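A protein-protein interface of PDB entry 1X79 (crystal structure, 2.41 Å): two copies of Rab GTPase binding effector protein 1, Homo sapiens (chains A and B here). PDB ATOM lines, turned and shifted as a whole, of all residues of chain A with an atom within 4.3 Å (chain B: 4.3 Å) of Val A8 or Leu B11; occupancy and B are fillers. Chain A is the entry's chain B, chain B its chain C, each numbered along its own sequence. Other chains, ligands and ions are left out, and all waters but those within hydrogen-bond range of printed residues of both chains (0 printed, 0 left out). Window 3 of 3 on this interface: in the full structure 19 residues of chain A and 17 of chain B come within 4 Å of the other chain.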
ATOM      1  N   THR A   4     -25.030  -3.380   3.033  1.00  0.00           N
ATOM      2  CA  THR A   4     -24.189  -4.122   2.090  1.00  0.00           C
ATOM      3  C   THR A   4     -24.044  -5.595   2.509  1.00  0.00           C
ATOM      4  O   THR A   4     -24.104  -6.497   1.673  1.00  0.00           O
ATOM      5  CB  THR A   4     -22.766  -3.467   1.949  1.00  0.00           C
ATOM      6  OG1 THR A   4     -22.735  -2.629   0.783  1.00  0.00           O
ATOM      7  CG2 THR A   4     -21.661  -4.529   1.841  1.00  0.00           C
ATOM      8  N   ARG A   5     -23.856  -5.836   3.802  1.00  0.00           N
ATOM      9  CA  ARG A   5     -23.778  -7.203   4.297  1.00  0.00           C
ATOM     10  C   ARG A   5     -24.947  -8.019   3.749  1.00  0.00           C
ATOM     11  O   ARG A   5     -24.771  -9.166   3.334  1.00  0.00           O
ATOM     12  CB  ARG A   5     -23.776  -7.208   5.832  1.00  0.00           C
ATOM     13  CG  ARG A   5     -22.522  -6.564   6.424  1.00  0.00           C
ATOM     14  CD  ARG A   5     -22.568  -6.434   7.948  1.00  0.00           C
ATOM     15  NE  ARG A   5     -21.357  -5.794   8.473  1.00  0.00           N
ATOM     16  CZ  ARG A   5     -21.164  -5.465   9.750  1.00  0.00           C
ATOM     17  NH1 ARG A   5     -22.106  -5.711  10.655  1.00  0.00           N
ATOM     18  NH2 ARG A   5     -20.024  -4.891  10.126  1.00  0.00           N
ATOM     19  N   ASP A   6     -26.130  -7.412   3.729  1.00  0.00           N
ATOM     20  CA  ASP A   6     -27.307  -8.067   3.190  1.00  0.00           C
ATOM     21  C   ASP A   6     -27.383  -8.003   1.684  1.00  0.00           C
ATOM     22  O   ASP A   6     -27.927  -8.895   1.051  1.00  0.00           O
ATOM     23  CB  ASP A   6     -28.556  -7.460   3.795  1.00  0.00           C
ATOM     24  CG  ASP A   6     -29.095  -8.300   4.926  1.00  0.00           C
ATOM     25  OD1 ASP A   6     -28.267  -8.860   5.689  1.00  0.00           O
ATOM     26  OD2 ASP A   6     -30.338  -8.401   5.049  1.00  0.00           O
ATOM     27  N   GLN A   7     -26.836  -6.936   1.117  1.00  0.00           N
ATOM     28  CA  GLN A   7     -26.631  -6.828  -0.318  1.00  0.00           C
ATOM     29  C   GLN A   7     -25.815  -8.025  -0.788  1.00  0.00           C
ATOM     30  O   GLN A   7     -26.249  -8.836  -1.610  1.00  0.00           O
ATOM     31  CB  GLN A   7     -25.848  -5.557  -0.622  1.00  0.00           C
ATOM     32  CG  GLN A   7     -26.435  -4.730  -1.711  1.00  0.00           C
ATOM     33  CD  GLN A   7     -27.784  -4.170  -1.338  1.00  0.00           C
ATOM     34  OE1 GLN A   7     -28.650  -4.884  -0.809  1.00  0.00           O
ATOM     35  NE2 GLN A   7     -27.983  -2.885  -1.623  1.00  0.00           N
ATOM     36  N   VAL A   8     -24.608  -8.124  -0.258  1.00  0.00           N
ATOM     37  CA  VAL A   8     -23.751  -9.240  -0.576  1.00  0.00           C
ATOM     38  C   VAL A   8     -24.410 -10.605  -0.319  1.00  0.00           C
ATOM     39  O   VAL A   8     -24.412 -11.468  -1.199  1.00  0.00           O
ATOM     40  CB  VAL A   8     -22.430  -9.096   0.179  1.00  0.00           C
ATOM     41  CG1 VAL A   8     -21.628 -10.402   0.140  1.00  0.00           C
ATOM     42  CG2 VAL A   8     -21.632  -7.988  -0.474  1.00  0.00           C
ATOM     43  N   LYS A   9     -24.991 -10.799   0.858  1.00  0.00           N
ATOM     44  CA  LYS A   9     -25.605 -12.087   1.153  1.00  0.00           C
ATOM     45  C   LYS A   9     -26.618 -12.498   0.091  1.00  0.00           C
ATOM     46  O   LYS A   9     -26.649 -13.650  -0.323  1.00  0.00           O
ATOM     47  CB  LYS A   9     -26.281 -12.081   2.530  1.00  0.00           C
ATOM     48  CG  LYS A   9     -26.359 -13.476   3.151  1.00  0.00           C
ATOM     49  CD  LYS A   9     -27.063 -13.499   4.520  1.00  0.00           C
ATOM     50  CE  LYS A   9     -28.596 -13.455   4.400  1.00  0.00           C
ATOM     51  NZ  LYS A   9     -29.303 -13.548   5.722  1.00  0.00           N
ATOM     52  N   LYS A  10     -27.442 -11.560  -0.354  1.00  0.00           N
ATOM     53  CA  LYS A  10     -28.528 -11.888  -1.286  1.00  0.00           C
ATOM     54  C   LYS A  10     -28.039 -12.134  -2.713  1.00  0.00           C
ATOM     55  O   LYS A  10     -28.542 -13.028  -3.390  1.00  0.00           O
ATOM     56  CB  LYS A  10     -29.583 -10.784  -1.293  1.00  0.00           C
ATOM     57  CG  LYS A  10     -30.345 -10.653   0.012  1.00  0.00           C
ATOM     58  CD  LYS A  10     -30.862  -9.232   0.158  1.00  0.00           C
ATOM     59  CE  LYS A  10     -31.495  -8.978   1.518  1.00  0.00           C
ATOM     60  NZ  LYS A  10     -32.756  -9.743   1.687  1.00  0.00           N
ATOM     61  N   LEU A  11     -27.066 -11.348  -3.166  1.00  0.00           N
ATOM     62  CA  LEU A  11     -26.334 -11.695  -4.352  1.00  0.00           C
ATOM     63  C   LEU A  11     -25.733 -13.112  -4.235  1.00  0.00           C
ATOM     64  O   LEU A  11     -25.866 -13.952  -5.134  1.00  0.00           O
ATOM     65  CB  LEU A  11     -25.253 -10.646  -4.616  1.00  0.00           C
ATOM     66  CG  LEU A  11     -25.797  -9.275  -5.098  1.00  0.00           C
ATOM     67  CD1 LEU A  11     -24.671  -8.298  -5.416  1.00  0.00           C
ATOM     68  CD2 LEU A  11     -26.589  -9.468  -6.361  1.00  0.00           C
ATOM     69  N   GLN A  12     -25.087 -13.420  -3.127  1.00  0.00           N
ATOM     70  CA  GLN A  12     -24.502 -14.742  -3.023  1.00  0.00           C
ATOM     71  C   GLN A  12     -25.586 -15.796  -3.189  1.00  0.00           C
ATOM     72  O   GLN A  12     -25.370 -16.865  -3.771  1.00  0.00           O
ATOM     73  CB  GLN A  12     -23.794 -14.884  -1.688  1.00  0.00           C
ATOM     74  CG  GLN A  12     -22.602 -13.976  -1.590  1.00  0.00           C
ATOM     75  CD  GLN A  12     -21.812 -14.195  -0.332  1.00  0.00           C
ATOM     76  OE1 GLN A  12     -22.395 -14.282   0.756  1.00  0.00           O
ATOM     77  NE2 GLN A  12     -20.471 -14.273  -0.457  1.00  0.00           N
ATOM     78  N   LEU A  15     -26.465 -16.235  -6.735  1.00  0.00           N
ATOM     79  CA  LEU A  15     -25.443 -16.973  -7.475  1.00  0.00           C
ATOM     80  C   LEU A  15     -25.681 -18.468  -7.288  1.00  0.00           C
ATOM     81  O   LEU A  15     -25.668 -19.221  -8.249  1.00  0.00           O
ATOM     82  CB  LEU A  15     -24.045 -16.597  -7.002  1.00  0.00           C
ATOM     83  CG  LEU A  15     -22.867 -16.866  -7.932  1.00  0.00           C
ATOM     84  CD1 LEU A  15     -23.011 -16.028  -9.185  1.00  0.00           C
ATOM     85  CD2 LEU A  15     -21.557 -16.488  -7.248  1.00  0.00           C
ATOM     86  N   GLN B   7     -17.088  -6.215  -3.526  1.00  0.00           N
ATOM     87  CA  GLN B   7     -17.845  -7.409  -3.222  1.00  0.00           C
ATOM     88  C   GLN B   7     -19.062  -7.475  -4.109  1.00  0.00           C
ATOM     89  O   GLN B   7     -19.199  -8.381  -4.919  1.00  0.00           O
ATOM     90  CB  GLN B   7     -18.297  -7.385  -1.786  1.00  0.00           C
ATOM     91  CG  GLN B   7     -17.190  -7.529  -0.792  1.00  0.00           C
ATOM     92  CD  GLN B   7     -17.570  -8.515   0.276  1.00  0.00           C
ATOM     93  OE1 GLN B   7     -17.578  -9.725   0.037  1.00  0.00           O
ATOM     94  NE2 GLN B   7     -17.923  -8.010   1.455  1.00  0.00           N
ATOM     95  N   VAL B   8     -19.948  -6.503  -3.945  1.00  0.00           N
ATOM     96  CA  VAL B   8     -21.127  -6.378  -4.785  1.00  0.00           C
ATOM     97  C   VAL B   8     -20.825  -6.296  -6.296  1.00  0.00           C
ATOM     98  O   VAL B   8     -21.416  -7.030  -7.085  1.00  0.00           O
ATOM     99  CB  VAL B   8     -21.965  -5.153  -4.361  1.00  0.00           C
ATOM    100  CG1 VAL B   8     -23.014  -4.858  -5.412  1.00  0.00           C
ATOM    101  CG2 VAL B   8     -22.645  -5.419  -3.006  1.00  0.00           C
ATOM    102  N   LYS B   9     -19.919  -5.420  -6.709  1.00  0.00           N
ATOM    103  CA  LYS B   9     -19.595  -5.342  -8.121  1.00  0.00           C
ATOM    104  C   LYS B   9     -19.094  -6.716  -8.595  1.00  0.00           C
ATOM    105  O   LYS B   9     -19.474  -7.215  -9.666  1.00  0.00           O
ATOM    106  CB  LYS B   9     -18.528  -4.274  -8.359  1.00  0.00           C
ATOM    107  CG  LYS B   9     -18.457  -3.786  -9.817  1.00  0.00           C
ATOM    108  CD  LYS B   9     -17.317  -2.762 -10.084  1.00  0.00           C
ATOM    109  CE  LYS B   9     -15.948  -3.429 -10.333  1.00  0.00           C
ATOM    110  NZ  LYS B   9     -15.864  -4.235 -11.603  1.00  0.00           N
ATOM    111  N   LYS B  10     -18.255  -7.329  -7.776  1.00  0.00           N
ATOM    112  CA  LYS B  10     -17.586  -8.573  -8.110  1.00  0.00           C
ATOM    113  C   LYS B  10     -18.567  -9.742  -8.271  1.00  0.00           C
ATOM    114  O   LYS B  10     -18.446 -10.536  -9.199  1.00  0.00           O
ATOM    115  CB  LYS B  10     -16.593  -8.880  -7.008  1.00  0.00           C
ATOM    116  CG  LYS B  10     -15.501  -9.845  -7.347  1.00  0.00           C
ATOM    117  CD  LYS B  10     -14.442  -9.770  -6.242  1.00  0.00           C
ATOM    118  CE  LYS B  10     -13.959  -8.318  -6.052  1.00  0.00           C
ATOM    119  NZ  LYS B  10     -13.110  -8.106  -4.840  1.00  0.00           N
ATOM    120  N   LEU B  11     -19.519  -9.856  -7.347  1.00  0.00           N
ATOM    121  CA  LEU B  11     -20.611 -10.803  -7.484  1.00  0.00           C
ATOM    122  C   LEU B  11     -21.513 -10.468  -8.675  1.00  0.00           C
ATOM    123  O   LEU B  11     -21.983 -11.353  -9.383  1.00  0.00           O
ATOM    124  CB  LEU B  11     -21.469 -10.831  -6.222  1.00  0.00           C
ATOM    125  CG  LEU B  11     -20.916 -11.484  -4.968  1.00  0.00           C
ATOM    126  CD1 LEU B  11     -21.714 -10.995  -3.787  1.00  0.00           C
ATOM    127  CD2 LEU B  11     -21.001 -12.977  -5.060  1.00  0.00           C
ATOM    128  N   GLN B  12     -21.791  -9.197  -8.891  1.00  0.00           N
ATOM    129  CA  GLN B  12     -22.629  -8.860 -10.021  1.00  0.00           C
ATOM    130  C   GLN B  12     -22.035  -9.398 -11.303  1.00  0.00           C
ATOM    131  O   GLN B  12     -22.760  -9.968 -12.095  1.00  0.00           O
ATOM    132  CB  GLN B  12     -22.829  -7.357 -10.110  1.00  0.00           C
ATOM    133  CG  GLN B  12     -23.804  -6.853  -9.057  1.00  0.00           C
ATOM    134  CD  GLN B  12     -23.983  -5.365  -9.104  1.00  0.00           C
ATOM    135  OE1 GLN B  12     -23.033  -4.603  -8.917  1.00  0.00           O
ATOM    136  NE2 GLN B  12     -25.208  -4.935  -9.357  1.00  0.00           N
ATOM    137  N   LEU B  13     -20.724  -9.255 -11.496  1.00  0.00           N
ATOM    138  CA  LEU B  13     -20.095  -9.744 -12.720  1.00  0.00           C
ATOM    139  C   LEU B  13     -20.113 -11.261 -12.818  1.00  0.00           C
ATOM    140  O   LEU B  13     -20.229 -11.823 -13.900  1.00  0.00           O
ATOM    141  CB  LEU B  13     -18.650  -9.259 -12.829  1.00  0.00           C
ATOM    142  CG  LEU B  13     -18.503  -7.735 -12.929  1.00  0.00           C
ATOM    143  CD1 LEU B  13     -17.037  -7.358 -13.015  1.00  0.00           C
ATOM    144  CD2 LEU B  13     -19.244  -7.212 -14.153  1.00  0.00           C
ATOM    145  N   MET B  14     -19.979 -11.926 -11.683  1.00  0.00           N
ATOM    146  CA  MET B  14     -20.112 -13.368 -11.648  1.00  0.00           C
ATOM    147  C   MET B  14     -21.552 -13.727 -12.011  1.00  0.00           C
ATOM    148  O   MET B  14     -21.784 -14.668 -12.762  1.00  0.00           O
ATOM    149  CB  MET B  14     -19.795 -13.889 -10.253  1.00  0.00           C
ATOM    150  CG  MET B  14     -18.374 -14.365 -10.021  1.00  0.00           C
ATOM    151  SD  MET B  14     -18.150 -15.023  -8.322  1.00  0.00           S
ATOM    152  CE  MET B  14     -18.196 -13.479  -7.468  1.00  0.00           C
ATOM    153  N   LEU B  15     -22.518 -12.984 -11.472  1.00  0.00           N
ATOM    154  CA  LEU B  15     -23.930 -13.326 -11.656  1.00  0.00           C
ATOM    155  C   LEU B  15     -24.312 -13.141 -13.126  1.00  0.00           C
ATOM    156  O   LEU B  15     -25.110 -13.883 -13.664  1.00  0.00           O
ATOM    157  CB  LEU B  15     -24.805 -12.409 -10.814  1.00  0.00           C
ATOM    158  CG  LEU B  15     -26.020 -12.932 -10.056  1.00  0.00           C
ATOM    159  CD1 LEU B  15     -27.100 -11.866 -10.148  1.00  0.00           C
ATOM    160  CD2 LEU B  15     -26.523 -14.226 -10.599  1.00  0.00           C
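Val A8 touches just these residues of chain B: Gln B7, Val B8 and Leu B11. Printed residues of chain A within 4 Å of Leu B11: Val A8 (3.8 Å), Leu A11 (3.7 Å) and Gln A12 (3.8 Å). Printed residues of chain B within 4 Å of Gln A12: Leu B11. Printed residues of chain A within 4 Å of Gln B7: Val A8. Of the printed residues of chain B, Gln A7 touches Val B8. Lys B10 touches none of the printed residues of chain A. The nearest printed residue of chain B that does not touch Val A8 is Lys B9 (7.0 Å). The nearest printed residue of chain B that does not touch Leu A15 is Leu B11 (4.2 Å).
Gln A7 touches Val B8. Val A8 touches Gln B7 (CG2 to CB, 3.6 Å). Val A8 touches Val B8 (CG2 to CG2, 3.7 Å). Leu B11 touches Val A8. CG1 of Val B8 touches CD1 of Leu A11, at 3.8 Å. Leu A11 touches Leu B11. CG of Gln A12 touches CD1 of Leu B11, at 3.8 Å. Met B14 touches Leu A15. CD1 of Leu A15 touches CA of Leu B15 (3.8 Å).
The side-chain amide oxygen of Gln B12 lies close to the backbone carbonyl oxygen of Val B8, at 3.4 Å.
Of the 10 printed residues of chain A, 5 touch a printed residue of chain B. Hydrophobic or aromatic side chains of chain A that line the printed part of chain B: Val A8, Leu A11 and Leu A15. Hydrophobic or aromatic side chains of chain B within 4 Å of the printed part of chain A: Val B8, Leu B11 and Met B14. Among the printed residues, no Asp or Glu carboxylate lies within 4 Å of a Lys or Arg side-chain nitrogen of the other chain.
Val A8 touches its own counterpart, Val B8. Val A8 touches Leu B11, and with the chains exchanged Leu A11 touches Val B8. Leu A11 touches its own counterpart, Leu B11. Leu B15 touches its own counterpart, Leu A15. 7 positions are printed for both chains. Of the 9 pairs that touch across the chains among the printed residues, 7 have their exchanged pair printed and touching as well.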
